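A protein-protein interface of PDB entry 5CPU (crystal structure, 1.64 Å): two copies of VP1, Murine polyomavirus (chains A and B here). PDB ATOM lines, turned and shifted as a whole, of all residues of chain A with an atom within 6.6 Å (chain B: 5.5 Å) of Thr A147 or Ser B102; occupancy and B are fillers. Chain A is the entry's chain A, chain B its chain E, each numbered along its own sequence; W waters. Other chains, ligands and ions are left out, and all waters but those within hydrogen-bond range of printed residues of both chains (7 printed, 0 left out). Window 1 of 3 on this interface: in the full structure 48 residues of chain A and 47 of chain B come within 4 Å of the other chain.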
ATOM      1  N   TYR A 130      -2.628  14.323  10.911  1.00  0.00           N
ATOM      2  CA  TYR A 130      -1.349  13.690  11.231  1.00  0.00           C
ATOM      3  C   TYR A 130      -1.638  12.457  12.060  1.00  0.00           C
ATOM      4  O   TYR A 130      -2.275  12.542  13.104  1.00  0.00           O
ATOM      5  CB  TYR A 130      -0.485  14.690  12.010  1.00  0.00           C
ATOM      6  CG  TYR A 130       0.961  14.303  12.230  1.00  0.00           C
ATOM      7  CD1 TYR A 130       1.836  14.121  11.150  1.00  0.00           C
ATOM      8  CD2 TYR A 130       1.463  14.158  13.530  1.00  0.00           C
ATOM      9  CE1 TYR A 130       3.169  13.791  11.359  1.00  0.00           C
ATOM     10  CE2 TYR A 130       2.796  13.826  13.752  1.00  0.00           C
ATOM     11  CZ  TYR A 130       3.641  13.647  12.666  1.00  0.00           C
ATOM     12  OH  TYR A 130       4.967  13.318  12.890  1.00  0.00           O
ATOM     13  N   LEU A 145      13.171  18.598  14.674  1.00  0.00           N
ATOM     14  CA  LEU A 145      13.240  19.417  13.457  1.00  0.00           C
ATOM     15  C   LEU A 145      12.053  20.361  13.519  1.00  0.00           C
ATOM     16  O   LEU A 145      10.915  19.915  13.715  1.00  0.00           O
ATOM     17  CB  LEU A 145      13.167  18.549  12.185  1.00  0.00           C
ATOM     18  CG  LEU A 145      13.333  19.268  10.832  1.00  0.00           C
ATOM     19  CD1 LEU A 145      13.829  18.261   9.805  1.00  0.00           C
ATOM     20  CD2 LEU A 145      12.059  19.960  10.341  1.00  0.00           C
ATOM     21  N   VAL A 146      12.321  21.661  13.368  1.00  0.00           N
ATOM     22  CA  VAL A 146      11.285  22.678  13.513  1.00  0.00           C
ATOM     23  C   VAL A 146      11.120  23.518  12.257  1.00  0.00           C
ATOM     24  O   VAL A 146      12.021  23.598  11.406  1.00  0.00           O
ATOM     25  CB  VAL A 146      11.570  23.628  14.713  1.00  0.00           C
ATOM     26  CG1 VAL A 146      11.523  22.857  16.036  1.00  0.00           C
ATOM     27  CG2 VAL A 146      12.909  24.347  14.560  1.00  0.00           C
ATOM     28  N   THR A 147       9.943  24.134  12.131  1.00  0.00           N
ATOM     29  CA  THR A 147       9.733  25.166  11.118  1.00  0.00           C
ATOM     30  C   THR A 147      10.702  26.338  11.292  1.00  0.00           C
ATOM     31  O   THR A 147      11.284  26.811  10.317  1.00  0.00           O
ATOM     32  CB  THR A 147       8.274  25.663  11.175  1.00  0.00           C
ATOM     33  OG1 THR A 147       7.443  24.673  10.551  1.00  0.00           O
ATOM     34  CG2 THR A 147       8.087  26.975  10.426  1.00  0.00           C
ATOM     35  N   ASP A 148      10.859  26.801  12.535  1.00  0.00           N
ATOM     36  CA  ASP A 148      11.582  28.039  12.803  1.00  0.00           C
ATOM     37  C   ASP A 148      12.396  27.897  14.093  1.00  0.00           C
ATOM     38  O   ASP A 148      11.835  27.772  15.191  1.00  0.00           O
ATOM     39  CB  ASP A 148      10.573  29.202  12.909  1.00  0.00           C
ATOM     40  CG  ASP A 148      11.233  30.587  12.950  1.00  0.00           C
ATOM     41  OD1 ASP A 148      12.456  30.699  13.159  1.00  0.00           O
ATOM     42  OD2 ASP A 148      10.497  31.583  12.764  1.00  0.00           O
ATOM     43  N   ALA A 149      13.721  27.893  13.945  1.00  0.00           N
ATOM     44  CA  ALA A 149      14.629  27.800  15.082  1.00  0.00           C
ATOM     45  C   ALA A 149      14.542  29.034  15.985  1.00  0.00           C
ATOM     46  O   ALA A 149      15.107  29.039  17.083  1.00  0.00           O
ATOM     47  CB  ALA A 149      16.060  27.618  14.588  1.00  0.00           C
ATOM     48  N   ARG A 150      13.837  30.072  15.534  1.00  0.00           N
ATOM     49  CA  ARG A 150      13.638  31.263  16.370  1.00  0.00           C
ATOM     50  C   ARG A 150      12.393  31.167  17.265  1.00  0.00           C
ATOM     51  O   ARG A 150      12.167  32.044  18.105  1.00  0.00           O
ATOM     52  CB  ARG A 150      13.567  32.526  15.510  1.00  0.00           C
ATOM     53  CG  ARG A 150      14.814  32.759  14.663  1.00  0.00           C
ATOM     54  CD  ARG A 150      14.572  33.810  13.589  1.00  0.00           C
ATOM     55  NE  ARG A 150      13.416  33.466  12.755  1.00  0.00           N
ATOM     56  CZ  ARG A 150      12.823  34.304  11.903  1.00  0.00           C
ATOM     57  NH1 ARG A 150      13.286  35.540  11.734  1.00  0.00           N
ATOM     58  NH2 ARG A 150      11.757  33.888  11.219  1.00  0.00           N
ATOM     59  N   THR A 151      11.576  30.131  17.074  1.00  0.00           N
ATOM     60  CA  THR A 151      10.339  30.009  17.862  1.00  0.00           C
ATOM     61  C   THR A 151      10.669  29.960  19.353  1.00  0.00           C
ATOM     62  O   THR A 151      11.553  29.202  19.782  1.00  0.00           O
ATOM     63  CB  THR A 151       9.543  28.762  17.452  1.00  0.00           C
ATOM     64  OG1 THR A 151       9.119  28.930  16.092  1.00  0.00           O
ATOM     65  CG2 THR A 151       8.315  28.581  18.364  1.00  0.00           C
ATOM     66  N   TYR A 153       9.568  28.673  22.221  1.00  0.00           N
ATOM     67  CA  TYR A 153       8.792  27.703  22.989  1.00  0.00           C
ATOM     68  C   TYR A 153       8.949  27.969  24.474  1.00  0.00           C
ATOM     69  O   TYR A 153      10.009  28.427  24.937  1.00  0.00           O
ATOM     70  CB  TYR A 153       9.259  26.283  22.682  1.00  0.00           C
ATOM     71  CG  TYR A 153       8.968  25.851  21.277  1.00  0.00           C
ATOM     72  CD1 TYR A 153       7.660  25.572  20.875  1.00  0.00           C
ATOM     73  CD2 TYR A 153       9.997  25.731  20.336  1.00  0.00           C
ATOM     74  CE1 TYR A 153       7.388  25.183  19.574  1.00  0.00           C
ATOM     75  CE2 TYR A 153       9.731  25.338  19.024  1.00  0.00           C
ATOM     76  CZ  TYR A 153       8.425  25.058  18.656  1.00  0.00           C
ATOM     77  OH  TYR A 153       8.146  24.664  17.362  1.00  0.00           O
ATOM     78  N   ASP A 173      18.617  23.221  13.085  1.00  0.00           N
ATOM     79  CA  ASP A 173      17.411  22.609  13.640  1.00  0.00           C
ATOM     80  C   ASP A 173      16.190  22.744  12.735  1.00  0.00           C
ATOM     81  O   ASP A 173      15.151  22.121  12.992  1.00  0.00           O
ATOM     82  CB  ASP A 173      17.126  23.168  15.039  1.00  0.00           C
ATOM     83  CG  ASP A 173      18.170  22.739  16.052  1.00  0.00           C
ATOM     84  OD1 ASP A 173      18.659  21.599  15.965  1.00  0.00           O
ATOM     85  OD2 ASP A 173      18.497  23.528  16.961  1.00  0.00           O
ATOM     86  N   GLN A 174      16.317  23.548  11.682  1.00  0.00           N
ATOM     87  CA  GLN A 174      15.282  23.632  10.649  1.00  0.00           C
ATOM     88  C   GLN A 174      15.455  22.542   9.591  1.00  0.00           C
ATOM     89  O   GLN A 174      14.570  22.335   8.745  1.00  0.00           O
ATOM     90  CB  GLN A 174      15.266  25.029  10.032  1.00  0.00           C
ATOM     91  CG  GLN A 174      14.891  26.082  11.074  1.00  0.00           C
ATOM     92  CD  GLN A 174      14.876  27.513  10.561  1.00  0.00           C
ATOM     93  OE1 GLN A 174      14.603  28.436  11.331  1.00  0.00           O
ATOM     94  NE2 GLN A 174      15.149  27.714   9.267  1.00  0.00           N
ATOM     95  N   VAL A 192       4.470  17.550  18.696  1.00  0.00           N
ATOM     96  CA  VAL A 192       4.621  16.863  17.411  1.00  0.00           C
ATOM     97  C   VAL A 192       5.160  17.755  16.289  1.00  0.00           C
ATOM     98  O   VAL A 192       5.642  17.251  15.269  1.00  0.00           O
ATOM     99  CB  VAL A 192       3.338  16.106  16.981  1.00  0.00           C
ATOM    100  CG1 VAL A 192       2.999  15.045  18.030  1.00  0.00           C
ATOM    101  CG2 VAL A 192       2.173  17.071  16.761  1.00  0.00           C
ATOM    102  N   GLU A 193       5.117  19.077  16.485  1.00  0.00           N
ATOM    103  CA  GLU A 193       5.690  19.983  15.491  1.00  0.00           C
ATOM    104  C   GLU A 193       7.210  20.117  15.690  1.00  0.00           C
ATOM    105  O   GLU A 193       7.884  20.773  14.899  1.00  0.00           O
ATOM    106  CB  GLU A 193       5.001  21.355  15.514  1.00  0.00           C
ATOM    107  CG  GLU A 193       5.368  22.246  16.702  1.00  0.00           C
ATOM    108  CD  GLU A 193       4.863  23.671  16.521  1.00  0.00           C
ATOM    109  OE1 GLU A 193       3.687  23.855  16.137  1.00  0.00           O
ATOM    110  OE2 GLU A 193       5.638  24.621  16.763  1.00  0.00           O
ATOM    111  N   ILE A 194       7.725  19.487  16.743  1.00  0.00           N
ATOM    112  CA  ILE A 194       9.168  19.498  17.030  1.00  0.00           C
ATOM    113  C   ILE A 194       9.793  18.115  16.883  1.00  0.00           C
ATOM    114  O   ILE A 194      10.875  17.977  16.320  1.00  0.00           O
ATOM    115  CB  ILE A 194       9.467  19.978  18.469  1.00  0.00           C
ATOM    116  CG1 ILE A 194       8.907  21.393  18.710  1.00  0.00           C
ATOM    117  CG2 ILE A 194      10.977  19.947  18.748  1.00  0.00           C
ATOM    118  CD1 ILE A 194       9.061  21.862  20.147  1.00  0.00           C
ATOM    119  N   HIS A 196      10.074  14.121  15.878  1.00  0.00           N
ATOM    120  CA  HIS A 196       9.709  13.146  14.839  1.00  0.00           C
ATOM    121  C   HIS A 196      10.350  11.811  15.142  1.00  0.00           C
ATOM    122  O   HIS A 196      11.382  11.760  15.792  1.00  0.00           O
ATOM    123  CB  HIS A 196      10.198  13.682  13.493  1.00  0.00           C
ATOM    124  CG  HIS A 196       9.924  15.138  13.353  1.00  0.00           C
ATOM    125  ND1 HIS A 196       8.648  15.618  13.173  1.00  0.00           N
ATOM    126  CD2 HIS A 196      10.716  16.218  13.545  1.00  0.00           C
ATOM    127  CE1 HIS A 196       8.675  16.940  13.193  1.00  0.00           C
ATOM    128  NE2 HIS A 196       9.918  17.327  13.424  1.00  0.00           N
ATOM    129  N   TYR A 211       1.043  12.171   6.942  1.00  0.00           N
ATOM    130  CA  TYR A 211       0.726  13.574   7.114  1.00  0.00           C
ATOM    131  C   TYR A 211      -0.030  14.022   5.870  1.00  0.00           C
ATOM    132  O   TYR A 211       0.347  13.665   4.753  1.00  0.00           O
ATOM    133  CB  TYR A 211       2.028  14.388   7.233  1.00  0.00           C
ATOM    134  CG  TYR A 211       1.827  15.878   7.088  1.00  0.00           C
ATOM    135  CD1 TYR A 211       1.374  16.643   8.158  1.00  0.00           C
ATOM    136  CD2 TYR A 211       2.049  16.525   5.866  1.00  0.00           C
ATOM    137  CE1 TYR A 211       1.172  18.008   8.030  1.00  0.00           C
ATOM    138  CE2 TYR A 211       1.836  17.893   5.734  1.00  0.00           C
ATOM    139  CZ  TYR A 211       1.399  18.620   6.820  1.00  0.00           C
ATOM    140  OH  TYR A 211       1.167  19.970   6.717  1.00  0.00           O
ATOM    141  N   TRP B  43      14.902  26.405   3.548  1.00  0.00           N
ATOM    142  CA  TRP B  43      13.967  27.127   2.688  1.00  0.00           C
ATOM    143  C   TRP B  43      14.707  27.827   1.545  1.00  0.00           C
ATOM    144  O   TRP B  43      15.928  27.986   1.588  1.00  0.00           O
ATOM    145  CB  TRP B  43      13.234  28.214   3.502  1.00  0.00           C
ATOM    146  CG  TRP B  43      12.620  27.733   4.800  1.00  0.00           C
ATOM    147  CD1 TRP B  43      13.274  27.523   5.988  1.00  0.00           C
ATOM    148  CD2 TRP B  43      11.236  27.431   5.040  1.00  0.00           C
ATOM    149  NE1 TRP B  43      12.378  27.089   6.953  1.00  0.00           N
ATOM    150  CE2 TRP B  43      11.124  27.025   6.396  1.00  0.00           C
ATOM    151  CE3 TRP B  43      10.079  27.461   4.237  1.00  0.00           C
ATOM    152  CZ2 TRP B  43       9.895  26.661   6.978  1.00  0.00           C
ATOM    153  CZ3 TRP B  43       8.858  27.087   4.812  1.00  0.00           C
ATOM    154  CH2 TRP B  43       8.778  26.692   6.171  1.00  0.00           C
ATOM    155  N   GLY B  99      10.498  14.915   9.201  1.00  0.00           N
ATOM    156  CA  GLY B  99      10.085  16.245   9.665  1.00  0.00           C
ATOM    157  C   GLY B  99       8.756  16.784   9.184  1.00  0.00           C
ATOM    158  O   GLY B  99       8.455  17.955   9.410  1.00  0.00           O
ATOM    159  N   SER B 100       7.937  15.963   8.525  1.00  0.00           N
ATOM    160  CA  SER B 100       6.635  16.467   8.082  1.00  0.00           C
ATOM    161  C   SER B 100       5.795  17.043   9.228  1.00  0.00           C
ATOM    162  O   SER B 100       5.051  18.008   9.030  1.00  0.00           O
ATOM    163  CB  SER B 100       5.844  15.415   7.278  1.00  0.00           C
ATOM    164  OG  SER B 100       5.580  14.262   8.049  1.00  0.00           O
ATOM    165  N   GLY B 101       5.924  16.471  10.421  1.00  0.00           N
ATOM    166  CA  GLY B 101       5.231  16.997  11.587  1.00  0.00           C
ATOM    167  C   GLY B 101       5.498  18.475  11.832  1.00  0.00           C
ATOM    168  O   GLY B 101       4.648  19.166  12.381  1.00  0.00           O
ATOM    169  N   SER B 102       6.667  18.965  11.417  1.00  0.00           N
ATOM    170  CA  SER B 102       6.986  20.391  11.619  1.00  0.00           C
ATOM    171  C   SER B 102       6.059  21.314  10.835  1.00  0.00           C
ATOM    172  O   SER B 102       5.934  22.505  11.161  1.00  0.00           O
ATOM    173  CB  SER B 102       8.449  20.698  11.253  1.00  0.00           C
ATOM    174  OG  SER B 102       8.657  20.600   9.847  1.00  0.00           O
ATOM    175  N   LEU B 103       5.406  20.776   9.804  1.00  0.00           N
ATOM    176  CA  LEU B 103       4.460  21.573   9.013  1.00  0.00           C
ATOM    177  C   LEU B 103       3.156  21.846   9.770  1.00  0.00           C
ATOM    178  O   LEU B 103       2.331  22.643   9.324  1.00  0.00           O
ATOM    179  CB  LEU B 103       4.184  20.890   7.667  1.00  0.00           C
ATOM    180  CG  LEU B 103       5.419  20.617   6.792  1.00  0.00           C
ATOM    181  CD1 LEU B 103       4.957  19.894   5.527  1.00  0.00           C
ATOM    182  CD2 LEU B 103       6.156  21.897   6.445  1.00  0.00           C
ATOM    183  N   LEU B 104       2.993  21.205  10.932  1.00  0.00           N
ATOM    184  CA  LEU B 104       1.852  21.458  11.818  1.00  0.00           C
ATOM    185  C   LEU B 104       2.014  22.751  12.617  1.00  0.00           C
ATOM    186  O   LEU B 104       1.135  23.117  13.399  1.00  0.00           O
ATOM    187  CB  LEU B 104       1.656  20.289  12.790  1.00  0.00           C
ATOM    188  CG  LEU B 104       1.354  18.950  12.103  1.00  0.00           C
ATOM    189  CD1 LEU B 104       1.556  17.792  13.073  1.00  0.00           C
ATOM    190  CD2 LEU B 104      -0.054  18.934  11.505  1.00  0.00           C
ATOM    191  N   ASP B 105       3.144  23.437  12.424  1.00  0.00           N
ATOM    192  CA  ASP B 105       3.311  24.776  12.998  1.00  0.00           C
ATOM    193  C   ASP B 105       2.499  25.764  12.167  1.00  0.00           C
ATOM    194  O   ASP B 105       2.912  26.157  11.067  1.00  0.00           O
ATOM    195  CB  ASP B 105       4.800  25.175  13.026  1.00  0.00           C
ATOM    196  CG  ASP B 105       5.018  26.661  13.373  1.00  0.00           C
ATOM    197  OD1 ASP B 105       4.050  27.403  13.623  1.00  0.00           O
ATOM    198  OD2 ASP B 105       6.194  27.086  13.400  1.00  0.00           O
ATOM    199  N   ARG B 268       9.928  25.107   0.716  1.00  0.00           N
ATOM    200  CA  ARG B 268      10.286  24.304   1.901  1.00  0.00           C
ATOM    201  C   ARG B 268      10.765  22.922   1.456  1.00  0.00           C
ATOM    202  O   ARG B 268      10.080  22.249   0.679  1.00  0.00           O
ATOM    203  CB  ARG B 268       9.088  24.151   2.864  1.00  0.00           C
ATOM    204  CG  ARG B 268       9.368  23.271   4.109  1.00  0.00           C
ATOM    205  CD  ARG B 268      10.641  23.685   4.862  1.00  0.00           C
ATOM    206  NE  ARG B 268      10.671  23.338   6.298  1.00  0.00           N
ATOM    207  CZ  ARG B 268      11.785  23.139   7.006  1.00  0.00           C
ATOM    208  NH1 ARG B 268      12.984  23.140   6.417  1.00  0.00           N
ATOM    209  NH2 ARG B 268      11.714  22.899   8.313  1.00  0.00           N
ATOM    210  N   LEU B 270      12.735  19.136   2.995  1.00  0.00           N
ATOM    211  CA  LEU B 270      12.982  18.339   4.188  1.00  0.00           C
ATOM    212  C   LEU B 270      14.129  17.363   3.953  1.00  0.00           C
ATOM    213  O   LEU B 270      14.368  16.961   2.802  1.00  0.00           O
ATOM    214  CB  LEU B 270      11.711  17.587   4.637  1.00  0.00           C
ATOM    215  CG  LEU B 270      10.591  18.427   5.262  1.00  0.00           C
ATOM    216  CD1 LEU B 270       9.380  17.545   5.536  1.00  0.00           C
ATOM    217  CD2 LEU B 270      11.037  19.120   6.551  1.00  0.00           C
HETATM  218  O   HOH W   1       0.019  21.319   8.667  1.00  0.00           O
HETATM  219  O   HOH W   2       5.044  25.720   9.302  1.00  0.00           O
HETATM  220  O   HOH W   3      10.962  29.329   9.231  1.00  0.00           O
HETATM  221  O   HOH W   4       8.872  26.393  14.751  1.00  0.00           O
HETATM  222  O   HOH W   5       1.543  22.237  16.357  1.00  0.00           O
HETATM  223  O   HOH W   6       8.772  23.025   8.581  1.00  0.00           O
HETATM  224  O   HOH W   7       7.146  14.005  11.393  1.00  0.00           O
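O of Val A146 sits at hydrogen-bond distance from NH2 of Arg B268 (3.2 Å).
NH1 of Arg B268 sits at hydrogen-bond distance from O of Gln A174 (2.9 Å).
The side-chain hydroxyl (OG1) of Thr A147 lies within hydrogen-bond range of the backbone carbonyl oxygen (O) of Ser B102, at 2.7 Å.
The backbone carbonyl oxygen (O) of Ile A194 lies within hydrogen-bond range of the backbone NH (N) of Leu A145 (2.9 Å).
OE1 of Gln A174 sits at hydrogen-bond distance from N of Ala A149, 2.8 Å away.
The backbone carbonyl oxygen (O) of Asp A173 sits at hydrogen-bond distance from the backbone NH (N) of Val A146, at 2.9 Å.
The side-chain hydroxyl (OH) of Tyr A153 sits at hydrogen-bond distance from the side-chain carboxylate (OE2) of Glu A193.
O of Gly B99 sits at hydrogen-bond distance from OG of Ser B102 (2.7 Å).
A ring nitrogen (NE2) of His A196 lies within hydrogen-bond range of the backbone carbonyl oxygen (O) of Ile A194, at 3.1 Å.
Among the printed residues, pairs that only touch across the chains: Glu A193 with Asp B105 (3.3 Å), Tyr A211 with Leu B103 (3.3 Å), His A196 with Ser B102 (3.4 Å), Thr A147 with Asp B105 (3.4 Å), Glu A193 with Gly B101 (3.4 Å), Glu A193 with Ser B102 (3.4 Å), Leu A145 with Ser B102 (3.5 Å), Thr A147 with Trp B43 (3.5 Å), Leu A145 with Arg B268 (3.6 Å), Val A192 with Gly B101 (3.6 Å), Tyr A130 with Leu B104 (3.6 Å), Tyr A211 with Ser B100 (3.6 Å), Gln A174 with Trp B43 (3.7 Å), His A196 with Gly B101 (3.8 Å), Tyr A211 with Leu B104 (3.8 Å), Val A192 with Leu B104 (3.8 Å), Glu A193 with Leu B104 (3.8 Å), Tyr A130 with Gly B101 (3.8 Å) and His A196 with Gly B99 (3.8 Å).
Of the printed residues of chain B, Tyr A130 touches Gly B101 (3.8 Å) and Leu B104 (3.6 Å).
Of the printed residues of chain B, Val A146 touches Arg B268.
Thr A147 touches just these residues of chain B: Trp B43 (3.5 Å), Ser B102 (2.7 Å) and Asp B105 (3.4 Å).
Of the printed residues of chain B, Val A192 touches Gly B101 (3.6 Å) and Leu B104 (3.8 Å).
Ile A194 touches none of the printed residues of chain B.
Of the printed residues of chain A, Ser B100 touches Tyr A211 (3.6 Å).
Of the printed residues of chain A, Ser B102 touches Leu A145, Thr A147, Glu A193 and His A196.
Leu B270 touches none of the printed residues of chain A.
The nearest printed residue of chain A that does not touch Ser B102 is Val A146 (4.01 Å).
The nearest printed residue of chain A that does not touch Trp B43 is Asp A148 (5.6 Å).
Hydrophobic or aromatic side chains of chain A within 4 Å of the printed part of chain B: Tyr A130, Leu A145, Val A192, His A196 and Tyr A211.
Printed residues of chain B that touch a printed residue of chain A: Trp B43, Gly B99, Ser B100, Gly B101, Ser B102, Leu B103, Leu B104, Asp B105 and Arg B268.
No position is printed for both chains.
Water W5 lies within hydrogen-bond range of the side-chain carboxylate (OE1) of Glu A193 (2.7 Å) and the backbone carbonyl oxygen (O) of Leu B104 (3.1 Å).
Water W7 lies within hydrogen-bond range of OH of Tyr A130 (2.7 Å), ND1 of His A196 (2.8 Å) and N of Gly B101 (2.9 Å).
Water W6 lies within hydrogen-bond range of OG of Ser B102 (2.7 Å), OG1 of Thr A147 (2.9 Å) and NH2 of Arg B268 (3.0 Å).
Water W3 lies within hydrogen-bond range of O of Thr A147 (2.8 Å) and NE1 of Trp B43 (3.5 Å).
Water W2 bridges the backbone carbonyl oxygen of Asp B105 (2.8 Å) and the side-chain hydroxyl of Thr A147 (2.9 Å).
Water W4 lies within hydrogen-bond range of the side-chain hydroxyl of Thr A151, the backbone NH of Asp A148, the side-chain carboxylate of Asp B105 and the side-chain hydroxyl of Tyr A153.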
